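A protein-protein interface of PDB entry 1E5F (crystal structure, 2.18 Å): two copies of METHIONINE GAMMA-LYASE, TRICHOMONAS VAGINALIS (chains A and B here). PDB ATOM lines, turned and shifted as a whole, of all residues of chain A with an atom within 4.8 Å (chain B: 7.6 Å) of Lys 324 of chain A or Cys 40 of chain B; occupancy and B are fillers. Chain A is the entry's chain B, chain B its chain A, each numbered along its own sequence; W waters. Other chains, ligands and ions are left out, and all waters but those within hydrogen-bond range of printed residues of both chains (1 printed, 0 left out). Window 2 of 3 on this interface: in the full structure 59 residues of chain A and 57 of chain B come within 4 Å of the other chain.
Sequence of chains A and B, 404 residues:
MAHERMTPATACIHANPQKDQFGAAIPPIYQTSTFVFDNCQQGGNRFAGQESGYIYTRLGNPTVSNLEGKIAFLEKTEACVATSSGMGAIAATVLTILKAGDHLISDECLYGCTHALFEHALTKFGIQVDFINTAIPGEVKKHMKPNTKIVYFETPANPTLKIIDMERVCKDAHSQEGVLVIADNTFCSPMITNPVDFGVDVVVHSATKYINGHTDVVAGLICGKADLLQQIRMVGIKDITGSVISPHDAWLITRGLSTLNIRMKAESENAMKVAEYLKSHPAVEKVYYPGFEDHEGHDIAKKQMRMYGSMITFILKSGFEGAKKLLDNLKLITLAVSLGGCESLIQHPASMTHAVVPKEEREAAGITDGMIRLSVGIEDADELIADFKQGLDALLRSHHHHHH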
ATOM      1  N   PHE A 320      -7.304  21.603   4.174  1.00  0.00           N
ATOM      2  CA  PHE A 320      -5.969  21.504   3.662  1.00  0.00           C
ATOM      3  C   PHE A 320      -4.865  22.037   4.552  1.00  0.00           C
ATOM      4  O   PHE A 320      -3.792  21.458   4.674  1.00  0.00           O
ATOM      5  CB  PHE A 320      -6.094  22.273   2.360  1.00  0.00           C
ATOM      6  CG  PHE A 320      -4.815  22.589   1.651  1.00  0.00           C
ATOM      7  CD1 PHE A 320      -4.231  21.620   0.865  1.00  0.00           C
ATOM      8  CD2 PHE A 320      -4.191  23.778   1.879  1.00  0.00           C
ATOM      9  CE1 PHE A 320      -2.994  21.919   0.272  1.00  0.00           C
ATOM     10  CE2 PHE A 320      -2.998  24.067   1.186  1.00  0.00           C
ATOM     11  CZ  PHE A 320      -2.405  23.161   0.370  1.00  0.00           C
ATOM     12  N   GLU A 321      -5.044  23.121   5.275  1.00  0.00           N
ATOM     13  CA  GLU A 321      -3.968  23.557   6.115  1.00  0.00           C
ATOM     14  C   GLU A 321      -3.916  22.578   7.293  1.00  0.00           C
ATOM     15  O   GLU A 321      -2.825  22.523   7.844  1.00  0.00           O
ATOM     16  CB  GLU A 321      -4.116  24.964   6.677  1.00  0.00           C
ATOM     17  CG  GLU A 321      -4.110  25.928   5.488  1.00  0.00           C
ATOM     18  CD  GLU A 321      -2.725  26.226   4.896  1.00  0.00           C
ATOM     19  OE1 GLU A 321      -1.716  26.093   5.627  1.00  0.00           O
ATOM     20  OE2 GLU A 321      -2.724  26.717   3.720  1.00  0.00           O
ATOM     21  N   GLY A 322      -5.123  22.107   7.754  1.00  0.00           N
ATOM     22  CA  GLY A 322      -5.003  21.146   8.841  1.00  0.00           C
ATOM     23  C   GLY A 322      -4.208  19.897   8.392  1.00  0.00           C
ATOM     24  O   GLY A 322      -3.344  19.330   9.064  1.00  0.00           O
ATOM     25  N   ALA A 323      -4.502  19.475   7.165  1.00  0.00           N
ATOM     26  CA  ALA A 323      -3.816  18.319   6.630  1.00  0.00           C
ATOM     27  C   ALA A 323      -2.286  18.535   6.686  1.00  0.00           C
ATOM     28  O   ALA A 323      -1.582  17.588   7.077  1.00  0.00           O
ATOM     29  CB  ALA A 323      -4.314  17.912   5.303  1.00  0.00           C
ATOM     30  N   LYS A 324      -1.791  19.735   6.298  1.00  0.00           N
ATOM     31  CA  LYS A 324      -0.371  19.922   6.231  1.00  0.00           C
ATOM     32  C   LYS A 324       0.206  19.887   7.620  1.00  0.00           C
ATOM     33  O   LYS A 324       1.322  19.354   7.814  1.00  0.00           O
ATOM     34  CB  LYS A 324       0.081  21.222   5.474  1.00  0.00           C
ATOM     35  CG  LYS A 324      -0.163  21.110   3.976  1.00  0.00           C
ATOM     36  CD  LYS A 324       0.454  22.281   3.161  1.00  0.00           C
ATOM     37  CE  LYS A 324      -0.346  23.567   3.454  1.00  0.00           C
ATOM     38  NZ  LYS A 324       0.478  24.753   3.084  1.00  0.00           N
ATOM     39  N   LYS A 325      -0.560  20.440   8.565  1.00  0.00           N
ATOM     40  CA  LYS A 325      -0.004  20.344   9.887  1.00  0.00           C
ATOM     41  C   LYS A 325       0.030  18.962  10.481  1.00  0.00           C
ATOM     42  O   LYS A 325       0.999  18.843  11.230  1.00  0.00           O
ATOM     43  CB  LYS A 325      -0.670  21.415  10.804  1.00  0.00           C
ATOM     44  N   LEU A 326      -1.071  18.262  10.382  1.00  0.00           N
ATOM     45  CA  LEU A 326      -1.003  16.902  10.885  1.00  0.00           C
ATOM     46  C   LEU A 326       0.230  16.227  10.301  1.00  0.00           C
ATOM     47  O   LEU A 326       1.096  15.770  11.027  1.00  0.00           O
ATOM     48  CB  LEU A 326      -2.180  16.040  10.375  1.00  0.00           C
ATOM     49  CG  LEU A 326      -2.137  14.655  10.966  1.00  0.00           C
ATOM     50  CD1 LEU A 326      -2.118  14.530  12.422  1.00  0.00           C
ATOM     51  CD2 LEU A 326      -3.432  13.983  10.452  1.00  0.00           C
ATOM     52  N   LEU A 327       0.238  16.131   8.951  1.00  0.00           N
ATOM     53  CA  LEU A 327       1.287  15.469   8.236  1.00  0.00           C
ATOM     54  C   LEU A 327       2.707  15.883   8.561  1.00  0.00           C
ATOM     55  O   LEU A 327       3.489  14.931   8.612  1.00  0.00           O
ATOM     56  CB  LEU A 327       1.201  15.311   6.694  1.00  0.00           C
ATOM     57  CG  LEU A 327      -0.123  14.816   6.138  1.00  0.00           C
ATOM     58  CD1 LEU A 327      -0.070  14.212   4.730  1.00  0.00           C
ATOM     59  CD2 LEU A 327      -0.900  13.964   7.008  1.00  0.00           C
ATOM     60  N   ASP A 328       3.018  17.137   8.641  1.00  0.00           N
ATOM     61  CA  ASP A 328       4.343  17.562   8.996  1.00  0.00           C
ATOM     62  C   ASP A 328       4.703  17.179  10.438  1.00  0.00           C
ATOM     63  O   ASP A 328       5.867  17.226  10.793  1.00  0.00           O
ATOM     64  CB  ASP A 328       4.412  19.184   8.920  1.00  0.00           C
ATOM     65  CG  ASP A 328       4.204  19.557   7.448  1.00  0.00           C
ATOM     66  OD1 ASP A 328       4.050  18.633   6.571  1.00  0.00           O
ATOM     67  OD2 ASP A 328       4.245  20.755   7.048  1.00  0.00           O
ATOM     68  N   LEU A 335       5.974  10.392   5.786  1.00  0.00           N
ATOM     69  CA  LEU A 335       5.424  11.176   4.668  1.00  0.00           C
ATOM     70  C   LEU A 335       6.042  10.766   3.340  1.00  0.00           C
ATOM     71  O   LEU A 335       7.088  11.307   2.938  1.00  0.00           O
ATOM     72  CB  LEU A 335       5.626  12.681   4.954  1.00  0.00           C
ATOM     73  CG  LEU A 335       4.951  13.668   3.995  1.00  0.00           C
ATOM     74  CD1 LEU A 335       3.450  13.491   4.008  1.00  0.00           C
ATOM     75  CD2 LEU A 335       5.299  15.110   4.434  1.00  0.00           C
ATOM     76  N   MET A 352      -0.027  15.718  -4.441  1.00  0.00           N
ATOM     77  CA  MET A 352       0.998  14.719  -4.679  1.00  0.00           C
ATOM     78  C   MET A 352       0.512  13.697  -5.673  1.00  0.00           C
ATOM     79  O   MET A 352       0.541  14.084  -6.869  1.00  0.00           O
ATOM     80  CB  MET A 352       1.541  14.275  -3.340  1.00  0.00           C
ATOM     81  CG  MET A 352       1.886  15.387  -2.252  1.00  0.00           C
ATOM     82  SD  MET A 352       2.128  14.440  -0.730  1.00  0.00           S
ATOM     83  CE  MET A 352       2.461  15.578   0.599  1.00  0.00           C
ATOM     84  N   PHE B  37       9.224  12.889   2.133  1.00  0.00           N
ATOM     85  CA  PHE B  37       9.297  14.345   2.118  1.00  0.00           C
ATOM     86  C   PHE B  37       9.627  14.753   3.522  1.00  0.00           C
ATOM     87  O   PHE B  37       9.015  14.286   4.488  1.00  0.00           O
ATOM     88  CB  PHE B  37       8.036  14.953   1.606  1.00  0.00           C
ATOM     89  CG  PHE B  37       7.732  14.500   0.169  1.00  0.00           C
ATOM     90  CD1 PHE B  37       8.664  14.601  -0.807  1.00  0.00           C
ATOM     91  CD2 PHE B  37       6.505  13.930  -0.081  1.00  0.00           C
ATOM     92  CE1 PHE B  37       8.345  14.204  -2.133  1.00  0.00           C
ATOM     93  CE2 PHE B  37       6.222  13.520  -1.393  1.00  0.00           C
ATOM     94  CZ  PHE B  37       7.130  13.635  -2.485  1.00  0.00           C
ATOM     95  N   ASP B  38      10.517  15.731   3.684  1.00  0.00           N
ATOM     96  CA  ASP B  38      10.632  16.500   4.890  1.00  0.00           C
ATOM     97  C   ASP B  38       9.353  17.179   5.434  1.00  0.00           C
ATOM     98  O   ASP B  38       9.092  17.217   6.638  1.00  0.00           O
ATOM     99  CB  ASP B  38      11.571  17.761   4.688  1.00  0.00           C
ATOM    100  CG  ASP B  38      12.982  17.176   4.529  1.00  0.00           C
ATOM    101  OD1 ASP B  38      13.290  16.065   5.026  1.00  0.00           O
ATOM    102  OD2 ASP B  38      13.791  17.863   3.873  1.00  0.00           O
ATOM    103  N   ASN B  39       8.526  17.709   4.538  1.00  0.00           N
ATOM    104  CA  ASN B  39       7.252  18.326   4.871  1.00  0.00           C
ATOM    105  C   ASN B  39       6.287  18.309   3.660  1.00  0.00           C
ATOM    106  O   ASN B  39       6.785  17.989   2.534  1.00  0.00           O
ATOM    107  CB  ASN B  39       7.447  19.739   5.408  1.00  0.00           C
ATOM    108  CG  ASN B  39       8.242  20.635   4.465  1.00  0.00           C
ATOM    109  OD1 ASN B  39       7.711  20.899   3.396  1.00  0.00           O
ATOM    110  ND2 ASN B  39       9.400  20.979   4.884  1.00  0.00           N
ATOM    111  N   CYS B  40       4.973  18.598   3.816  1.00  0.00           N
ATOM    112  CA  CYS B  40       4.021  18.550   2.714  1.00  0.00           C
ATOM    113  C   CYS B  40       4.346  19.514   1.605  1.00  0.00           C
ATOM    114  O   CYS B  40       4.193  19.180   0.399  1.00  0.00           O
ATOM    115  CB  CYS B  40       2.557  18.878   3.126  1.00  0.00           C
ATOM    116  SG  CYS B  40       1.956  17.499   4.138  1.00  0.00           S
ATOM    117  N   GLN B  41       4.759  20.702   1.982  1.00  0.00           N
ATOM    118  CA  GLN B  41       5.156  21.703   0.961  1.00  0.00           C
ATOM    119  C   GLN B  41       6.224  21.235  -0.037  1.00  0.00           C
ATOM    120  O   GLN B  41       6.050  21.409  -1.252  1.00  0.00           O
ATOM    121  CB  GLN B  41       5.842  22.873   1.667  1.00  0.00           C
ATOM    122  CG  GLN B  41       4.952  24.084   1.849  1.00  0.00           C
ATOM    123  CD  GLN B  41       4.859  24.696   0.443  1.00  0.00           C
ATOM    124  OE1 GLN B  41       3.820  24.736  -0.205  1.00  0.00           O
ATOM    125  NE2 GLN B  41       6.093  25.033   0.127  1.00  0.00           N
ATOM    126  N   GLN B  42       7.313  20.674   0.524  1.00  0.00           N
ATOM    127  CA  GLN B  42       8.383  20.132  -0.332  1.00  0.00           C
ATOM    128  C   GLN B  42       7.829  19.072  -1.285  1.00  0.00           C
ATOM    129  O   GLN B  42       7.997  19.116  -2.507  1.00  0.00           O
ATOM    130  CB  GLN B  42       9.434  19.568   0.625  1.00  0.00           C
ATOM    131  CG  GLN B  42      10.608  18.925  -0.200  1.00  0.00           C
ATOM    132  CD  GLN B  42      11.622  18.319   0.758  1.00  0.00           C
ATOM    133  OE1 GLN B  42      11.389  17.212   1.236  1.00  0.00           O
ATOM    134  NE2 GLN B  42      12.714  18.981   1.145  1.00  0.00           N
ATOM    135  N   GLY B  43       6.915  18.217  -0.833  1.00  0.00           N
ATOM    136  CA  GLY B  43       6.229  17.218  -1.601  1.00  0.00           C
ATOM    137  C   GLY B  43       5.512  17.884  -2.796  1.00  0.00           C
ATOM    138  O   GLY B  43       5.689  17.446  -3.942  1.00  0.00           O
ATOM    139  N   GLY B  44       4.665  18.872  -2.564  1.00  0.00           N
ATOM    140  CA  GLY B  44       3.850  19.603  -3.573  1.00  0.00           C
ATOM    141  C   GLY B  44       4.809  20.378  -4.532  1.00  0.00           C
ATOM    142  O   GLY B  44       4.615  20.277  -5.740  1.00  0.00           O
ATOM    143  N   ASN B  45       5.873  20.892  -3.939  1.00  0.00           N
ATOM    144  CA  ASN B  45       6.837  21.593  -4.751  1.00  0.00           C
ATOM    145  C   ASN B  45       7.550  20.696  -5.765  1.00  0.00           C
ATOM    146  O   ASN B  45       7.788  21.080  -6.889  1.00  0.00           O
ATOM    147  CB  ASN B  45       7.912  22.273  -3.856  1.00  0.00           C
ATOM    148  CG  ASN B  45       7.451  23.497  -3.107  1.00  0.00           C
ATOM    149  OD1 ASN B  45       6.361  24.036  -3.347  1.00  0.00           O
ATOM    150  ND2 ASN B  45       8.296  23.868  -2.172  1.00  0.00           N
ATOM    151  N   ARG B  46       7.999  19.549  -5.240  1.00  0.00           N
ATOM    152  CA  ARG B  46       8.682  18.577  -6.072  1.00  0.00           C
ATOM    153  C   ARG B  46       7.671  18.214  -7.151  1.00  0.00           C
ATOM    154  O   ARG B  46       8.008  18.205  -8.339  1.00  0.00           O
ATOM    155  CB  ARG B  46       9.035  17.407  -5.193  1.00  0.00           C
ATOM    156  CG  ARG B  46      10.386  16.976  -4.727  1.00  0.00           C
ATOM    157  CD  ARG B  46      10.888  17.606  -3.535  1.00  0.00           C
ATOM    158  NE  ARG B  46      11.919  16.891  -2.850  1.00  0.00           N
ATOM    159  CZ  ARG B  46      12.834  16.259  -2.242  1.00  0.00           C
ATOM    160  NH1 ARG B  46      14.033  16.676  -1.780  1.00  0.00           N
ATOM    161  NH2 ARG B  46      12.341  15.066  -1.764  1.00  0.00           N
ATOM    162  N   PHE B  47       6.453  17.786  -6.771  1.00  0.00           N
ATOM    163  CA  PHE B  47       5.490  17.396  -7.831  1.00  0.00           C
ATOM    164  C   PHE B  47       5.219  18.490  -8.870  1.00  0.00           C
ATOM    165  O   PHE B  47       4.682  18.139  -9.917  1.00  0.00           O
ATOM    166  CB  PHE B  47       4.108  17.077  -7.196  1.00  0.00           C
ATOM    167  CG  PHE B  47       3.986  15.587  -6.922  1.00  0.00           C
ATOM    168  CD1 PHE B  47       3.797  14.724  -7.990  1.00  0.00           C
ATOM    169  CD2 PHE B  47       4.346  15.085  -5.670  1.00  0.00           C
ATOM    170  CE1 PHE B  47       3.794  13.341  -7.767  1.00  0.00           C
ATOM    171  CE2 PHE B  47       4.292  13.714  -5.480  1.00  0.00           C
ATOM    172  CZ  PHE B  47       4.065  12.827  -6.511  1.00  0.00           C
HETATM  173  O   HOH W   1       4.386  21.720   4.540  1.00  0.00           O
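Cys 40 of chain B touches Lys 324 of chain A (CB to CG, 3.6 Å). Leu 327 of chain A touches Cys 40 of chain B (CB to SG, 3.4 Å). Asn 39 of chain B touches Asp 328 of chain A (CA to OD1, 3.6 Å). Asn 39 of chain B touches Leu 335 of chain A (C to CD2, 3.4 Å). Leu 335 of chain A touches Cys 40 of chain B. CA of Cys 40 of chain B touches CE of Met 352 of chain A, 3.97 Å away. Met 352 of chain A touches Phe 47 of chain B (O to CE1, 3.5 Å).
Of the printed residues of chain B, Leu 327 of chain A touches Cys 40. Of the printed residues of chain B, Asp 328 of chain A touches Asn 39 and Cys 40. Printed residues of chain B within 4 Å of Met 352 of chain A: Cys 40 (3.97 Å) and Phe 47 (3.5 Å). Printed residues of chain A within 4 Å of Phe 37 of chain B: Leu 335. Printed residues of chain A within 4 Å of Asn 39 of chain B: Asp 328 and Leu 335. Of the printed residues of chain A, Cys 40 of chain B touches Lys 324 (3.6 Å), Leu 327 (3.4 Å), Asp 328 (2.9 Å), Leu 335 (3.6 Å) and Met 352 (3.97 Å). The nearest residue of chain A that does not touch Cys 40 of chain B is Ala 323 of chain A (4.6 Å).
Water W1 lies within hydrogen-bond range of the side-chain carboxylate of Asp 328 of chain A, the backbone NH of Gln 41 of chain B and the backbone NH of Cys 40 of chain B.
No position is printed for both chains. Of the 9 pairs that touch across the chains among the printed residues, none has its exchanged pair printed and touching as well.
N of Cys 40 of chain B sits at hydrogen-bond distance from OD1 of Asp 328 of chain A (2.9 Å). The backbone NH of Phe 37 of chain B is in hydrogen-bond range of the backbone carbonyl oxygen of Leu 335 of chain A (2.8 Å).
Hydrophobic or aromatic side chains of chain A that line the printed part of chain B: Leu 327, Leu 335 and Met 352. Of the 11 printed residues of chain B, 4 touch a printed residue of chain A. Printed residues of chain B that touch a printed residue of chain A: Phe 37, Asn 39, Cys 40 and Phe 47. Hydrophobic or aromatic side chains of chain B within 4 Å of the printed part of chain A: Phe 37 and Phe 47. Among the printed residues, 9 pairs touch across the chains. Among the printed residues, no Asp or Glu carboxylate lies within 4 Å of a Lys or Arg side-chain nitrogen of the other chain.
The side-chain amide oxygen of Asn 39 of chain B sits at hydrogen-bond distance from the backbone NH of Gln 42 of chain B (2.9 Å). NZ of Lys 324 of chain A is in salt-bridge range of OE1 of Glu 321 of chain A (3.6 Å). N of Gln 41 of chain B sits close to OD1 of Asn 39 of chain B, at 3.3 Å.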
